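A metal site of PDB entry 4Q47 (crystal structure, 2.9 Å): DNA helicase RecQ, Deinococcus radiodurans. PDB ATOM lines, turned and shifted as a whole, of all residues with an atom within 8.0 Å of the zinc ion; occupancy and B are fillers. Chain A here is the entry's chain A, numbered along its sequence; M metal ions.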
ATOM      1  N   TYR A 214      -5.219 -22.526  25.667  1.00  0.00           N
ATOM      2  CA  TYR A 214      -4.295 -22.508  24.546  1.00  0.00           C
ATOM      3  C   TYR A 214      -4.960 -22.132  23.224  1.00  0.00           C
ATOM      4  O   TYR A 214      -6.012 -22.647  22.879  1.00  0.00           O
ATOM      5  CB  TYR A 214      -3.630 -23.859  24.416  1.00  0.00           C
ATOM      6  CG  TYR A 214      -2.846 -24.241  25.610  1.00  0.00           C
ATOM      7  CD1 TYR A 214      -3.448 -24.922  26.658  1.00  0.00           C
ATOM      8  CD2 TYR A 214      -1.496 -23.936  25.717  1.00  0.00           C
ATOM      9  CE1 TYR A 214      -2.735 -25.281  27.780  1.00  0.00           C
ATOM     10  CE2 TYR A 214      -0.773 -24.300  26.831  1.00  0.00           C
ATOM     11  CZ  TYR A 214      -1.404 -24.973  27.859  1.00  0.00           C
ATOM     12  OH  TYR A 214      -0.704 -25.338  28.981  1.00  0.00           O
ATOM     13  N   THR A 380      -7.601 -31.257  16.067  1.00  0.00           N
ATOM     14  CA  THR A 380      -8.201 -31.857  17.267  1.00  0.00           C
ATOM     15  C   THR A 380      -7.629 -31.186  18.503  1.00  0.00           C
ATOM     16  O   THR A 380      -6.640 -30.433  18.393  1.00  0.00           O
ATOM     17  CB  THR A 380      -7.943 -33.408  17.357  1.00  0.00           C
ATOM     18  OG1 THR A 380      -6.600 -33.666  17.824  1.00  0.00           O
ATOM     19  CG2 THR A 380      -8.151 -34.093  16.022  1.00  0.00           C
ATOM     20  N   CYS A 381      -8.195 -31.493  19.670  1.00  0.00           N
ATOM     21  CA  CYS A 381      -7.918 -30.764  20.918  1.00  0.00           C
ATOM     22  C   CYS A 381      -6.441 -30.537  21.170  1.00  0.00           C
ATOM     23  O   CYS A 381      -5.648 -31.462  21.122  1.00  0.00           O
ATOM     24  CB  CYS A 381      -8.502 -31.514  22.111  1.00  0.00           C
ATOM     25  SG  CYS A 381      -7.974 -30.897  23.766  1.00  0.00           S
ATOM     26  N   ARG A 382      -6.090 -29.290  21.444  1.00  0.00           N
ATOM     27  CA  ARG A 382      -4.683 -28.902  21.458  1.00  0.00           C
ATOM     28  C   ARG A 382      -3.990 -29.382  22.696  1.00  0.00           C
ATOM     29  O   ARG A 382      -2.781 -29.554  22.699  1.00  0.00           O
ATOM     30  CB  ARG A 382      -4.527 -27.386  21.449  1.00  0.00           C
ATOM     31  CG  ARG A 382      -4.714 -26.733  20.140  1.00  0.00           C
ATOM     32  CD  ARG A 382      -4.067 -25.378  20.167  1.00  0.00           C
ATOM     33  NE  ARG A 382      -4.248 -24.766  18.856  1.00  0.00           N
ATOM     34  CZ  ARG A 382      -3.631 -25.163  17.748  1.00  0.00           C
ATOM     35  NH1 ARG A 382      -2.773 -26.173  17.792  1.00  0.00           N
ATOM     36  NH2 ARG A 382      -3.877 -24.553  16.604  1.00  0.00           N
ATOM     37  N   ARG A 383      -4.773 -29.592  23.738  1.00  0.00           N
ATOM     38  CA  ARG A 383      -4.182 -29.969  25.001  1.00  0.00           C
ATOM     39  C   ARG A 383      -3.716 -31.439  24.899  1.00  0.00           C
ATOM     40  O   ARG A 383      -2.665 -31.778  25.420  1.00  0.00           O
ATOM     41  CB  ARG A 383      -5.158 -29.754  26.142  1.00  0.00           C
ATOM     42  CG  ARG A 383      -4.469 -29.341  27.410  1.00  0.00           C
ATOM     43  CD  ARG A 383      -5.442 -29.205  28.556  1.00  0.00           C
ATOM     44  NE  ARG A 383      -6.189 -27.953  28.501  1.00  0.00           N
ATOM     45  CZ  ARG A 383      -5.794 -26.816  29.058  1.00  0.00           C
ATOM     46  NH1 ARG A 383      -4.654 -26.743  29.720  1.00  0.00           N
ATOM     47  NH2 ARG A 383      -6.567 -25.756  28.955  1.00  0.00           N
ATOM     48  N   GLN A 384      -4.473 -32.272  24.205  1.00  0.00           N
ATOM     49  CA  GLN A 384      -4.061 -33.650  23.997  1.00  0.00           C
ATOM     50  C   GLN A 384      -2.770 -33.742  23.197  1.00  0.00           C
ATOM     51  O   GLN A 384      -1.838 -34.465  23.582  1.00  0.00           O
ATOM     52  CB  GLN A 384      -5.140 -34.424  23.253  1.00  0.00           C
ATOM     53  CG  GLN A 384      -6.346 -34.742  24.094  1.00  0.00           C
ATOM     54  CD  GLN A 384      -7.491 -35.308  23.278  1.00  0.00           C
ATOM     55  OE1 GLN A 384      -7.533 -35.128  22.054  1.00  0.00           O
ATOM     56  NE2 GLN A 384      -8.429 -35.971  23.941  1.00  0.00           N
ATOM     57  N   VAL A 385      -2.668 -32.952  22.132  1.00  0.00           N
ATOM     58  CA  VAL A 385      -1.470 -32.934  21.314  1.00  0.00           C
ATOM     59  C   VAL A 385      -0.258 -32.537  22.127  1.00  0.00           C
ATOM     60  O   VAL A 385       0.777 -33.196  22.076  1.00  0.00           O
ATOM     61  CB  VAL A 385      -1.580 -31.934  20.171  1.00  0.00           C
ATOM     62  CG1 VAL A 385      -0.314 -31.968  19.325  1.00  0.00           C
ATOM     63  CG2 VAL A 385      -2.787 -32.223  19.320  1.00  0.00           C
ATOM     64  N   LEU A 394      -4.530 -37.537  27.632  1.00  0.00           N
ATOM     65  CA  LEU A 394      -5.770 -36.949  28.088  1.00  0.00           C
ATOM     66  C   LEU A 394      -6.889 -37.665  27.342  1.00  0.00           C
ATOM     67  O   LEU A 394      -6.932 -37.633  26.112  1.00  0.00           O
ATOM     68  CB  LEU A 394      -5.775 -35.446  27.846  1.00  0.00           C
ATOM     69  CG  LEU A 394      -6.876 -34.653  28.544  1.00  0.00           C
ATOM     70  CD1 LEU A 394      -6.891 -34.982  30.006  1.00  0.00           C
ATOM     71  CD2 LEU A 394      -6.684 -33.171  28.326  1.00  0.00           C
ATOM     72  N   GLU A 396     -10.276 -37.324  27.122  1.00  0.00           N
ATOM     73  CA  GLU A 396     -11.259 -36.526  26.417  1.00  0.00           C
ATOM     74  C   GLU A 396     -10.768 -35.109  26.158  1.00  0.00           C
ATOM     75  O   GLU A 396      -9.909 -34.600  26.896  1.00  0.00           O
ATOM     76  CB  GLU A 396     -12.564 -36.498  27.215  1.00  0.00           C
ATOM     77  CG  GLU A 396     -13.110 -37.863  27.607  1.00  0.00           C
ATOM     78  CD  GLU A 396     -13.174 -38.848  26.443  1.00  0.00           C
ATOM     79  OE1 GLU A 396     -14.067 -38.707  25.578  1.00  0.00           O
ATOM     80  OE2 GLU A 396     -12.334 -39.771  26.407  1.00  0.00           O
ATOM     81  N   PRO A 397     -11.295 -34.451  25.102  1.00  0.00           N
ATOM     82  CA  PRO A 397     -10.998 -33.052  24.761  1.00  0.00           C
ATOM     83  C   PRO A 397     -11.185 -32.090  25.946  1.00  0.00           C
ATOM     84  O   PRO A 397     -12.093 -32.247  26.763  1.00  0.00           O
ATOM     85  CB  PRO A 397     -11.999 -32.768  23.646  1.00  0.00           C
ATOM     86  CG  PRO A 397     -12.109 -34.060  22.939  1.00  0.00           C
ATOM     87  CD  PRO A 397     -12.064 -35.104  24.034  1.00  0.00           C
ATOM     88  N   CYS A 398     -10.318 -31.098  26.038  1.00  0.00           N
ATOM     89  CA  CYS A 398     -10.226 -30.366  27.289  1.00  0.00           C
ATOM     90  C   CYS A 398     -11.385 -29.409  27.473  1.00  0.00           C
ATOM     91  O   CYS A 398     -11.833 -29.207  28.605  1.00  0.00           O
ATOM     92  CB  CYS A 398      -8.895 -29.626  27.365  1.00  0.00           C
ATOM     93  SG  CYS A 398      -8.693 -28.284  26.177  1.00  0.00           S
ATOM     94  N   GLY A 399     -11.865 -28.825  26.376  1.00  0.00           N
ATOM     95  CA  GLY A 399     -12.913 -27.812  26.456  1.00  0.00           C
ATOM     96  C   GLY A 399     -12.359 -26.454  26.864  1.00  0.00           C
ATOM     97  O   GLY A 399     -13.081 -25.476  27.010  1.00  0.00           O
ATOM     98  N   ASN A 400     -11.078 -26.427  27.176  1.00  0.00           N
ATOM     99  CA  ASN A 400     -10.369 -25.178  27.393  1.00  0.00           C
ATOM    100  C   ASN A 400      -9.414 -24.710  26.260  1.00  0.00           C
ATOM    101  O   ASN A 400      -8.490 -23.930  26.552  1.00  0.00           O
ATOM    102  CB  ASN A 400      -9.627 -25.218  28.725  1.00  0.00           C
ATOM    103  CG  ASN A 400      -9.548 -23.845  29.352  1.00  0.00           C
ATOM    104  OD1 ASN A 400     -10.311 -22.943  28.986  1.00  0.00           O
ATOM    105  ND2 ASN A 400      -8.613 -23.674  30.284  1.00  0.00           N
ATOM    106  N   CYS A 401      -9.481 -25.261  25.050  1.00  0.00           N
ATOM    107  CA  CYS A 401      -8.598 -24.714  24.009  1.00  0.00           C
ATOM    108  C   CYS A 401      -9.330 -24.131  22.792  1.00  0.00           C
ATOM    109  O   CYS A 401     -10.540 -24.279  22.642  1.00  0.00           O
ATOM    110  CB  CYS A 401      -7.567 -25.778  23.559  1.00  0.00           C
ATOM    111  SG  CYS A 401      -8.151 -27.137  22.479  1.00  0.00           S
ATOM    112  N   ASP A 402      -8.577 -23.482  21.890  1.00  0.00           N
ATOM    113  CA  ASP A 402      -9.177 -22.779  20.770  1.00  0.00           C
ATOM    114  C   ASP A 402      -9.805 -23.724  19.752  1.00  0.00           C
ATOM    115  O   ASP A 402     -10.716 -23.329  19.026  1.00  0.00           O
ATOM    116  CB  ASP A 402      -8.143 -21.848  20.098  1.00  0.00           C
ATOM    117  CG  ASP A 402      -7.104 -22.582  19.229  1.00  0.00           C
ATOM    118  OD1 ASP A 402      -6.402 -21.890  18.460  1.00  0.00           O
ATOM    119  OD2 ASP A 402      -6.953 -23.814  19.311  1.00  0.00           O
ATOM    120  N   VAL A 403      -9.314 -24.969  19.701  1.00  0.00           N
ATOM    121  CA  VAL A 403      -9.851 -25.999  18.809  1.00  0.00           C
ATOM    122  C   VAL A 403     -11.113 -26.589  19.374  1.00  0.00           C
ATOM    123  O   VAL A 403     -12.073 -26.835  18.659  1.00  0.00           O
ATOM    124  CB  VAL A 403      -8.846 -27.137  18.577  1.00  0.00           C
ATOM    125  CG1 VAL A 403      -9.482 -28.234  17.724  1.00  0.00           C
ATOM    126  CG2 VAL A 403      -7.599 -26.616  17.912  1.00  0.00           C
ATOM    127  N   CYS A 404     -11.092 -26.830  20.674  1.00  0.00           N
ATOM    128  CA  CYS A 404     -12.241 -27.350  21.405  1.00  0.00           C
ATOM    129  C   CYS A 404     -13.399 -26.382  21.291  1.00  0.00           C
ATOM    130  O   CYS A 404     -14.471 -26.737  20.791  1.00  0.00           O
ATOM    131  CB  CYS A 404     -11.872 -27.600  22.883  1.00  0.00           C
ATOM    132  SG  CYS A 404     -11.231 -29.240  23.126  1.00  0.00           S
ATOM    133  N   LEU A 405     -13.147 -25.152  21.711  1.00  0.00           N
ATOM    134  CA  LEU A 405     -14.173 -24.118  21.819  1.00  0.00           C
ATOM    135  C   LEU A 405     -14.675 -23.597  20.480  1.00  0.00           C
ATOM    136  O   LEU A 405     -15.861 -23.357  20.337  1.00  0.00           O
ATOM    137  CB  LEU A 405     -13.623 -22.951  22.637  1.00  0.00           C
ATOM    138  CG  LEU A 405     -13.322 -23.360  24.078  1.00  0.00           C
ATOM    139  CD1 LEU A 405     -12.586 -22.278  24.783  1.00  0.00           C
ATOM    140  CD2 LEU A 405     -14.608 -23.701  24.803  1.00  0.00           C
HETATM  141 ZN    ZN M   1      -9.015 -28.757  23.878  1.00  0.00          ZN
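The backbone NH of Arg 382 lies close to the side-chain sulfur of Cys 401, at 3.2 Å.
SG of Cys 401 lies close to N of Val 403 (3.7 Å).
The side-chain sulfur (SG) of Cys 398 sits close to the guanidinium group (NE) of Arg 383 (3.4 Å).
The backbone NH (N) of Asn 400 sits close to the side-chain sulfur (SG) of Cys 398, 3.2 Å away.
The side-chain sulfur (SG) of Cys 381 lies close to the backbone NH (N) of Arg 383 (3.5 Å).
The side-chain sulfur (SG) of Cys 381 lies close to the backbone NH (N) of Gln 384, 3.8 Å away.
N of Gly 399 sits close to SG of Cys 404.
The side-chain carboxylate of Asp 402 is in salt-bridge range of the guanidinium group of Arg 382, 2.9 Å away.
Residues that only touch the zinc ion: Gly 399 (3.8 Å) and Arg 382 (3.8 Å).
Within 4 Å of the zinc ion: Cys 381, Arg 382, Cys 398, Gly 399, Cys 401 and Cys 404.
The nearest printed residue that does not touch the zinc ion is Arg 383 (4.3 Å).
SG of Cys 401 binds the zinc ion, 2.3 Å away.
SG of Cys 398 binds the zinc ion, at 2.4 Å.
The zinc ion is bound by SG of Cys 381 (2.4 Å).
The zinc ion is bound by SG of Cys 404 (2.4 Å).
The zinc ion has four donor atoms within binding distance.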
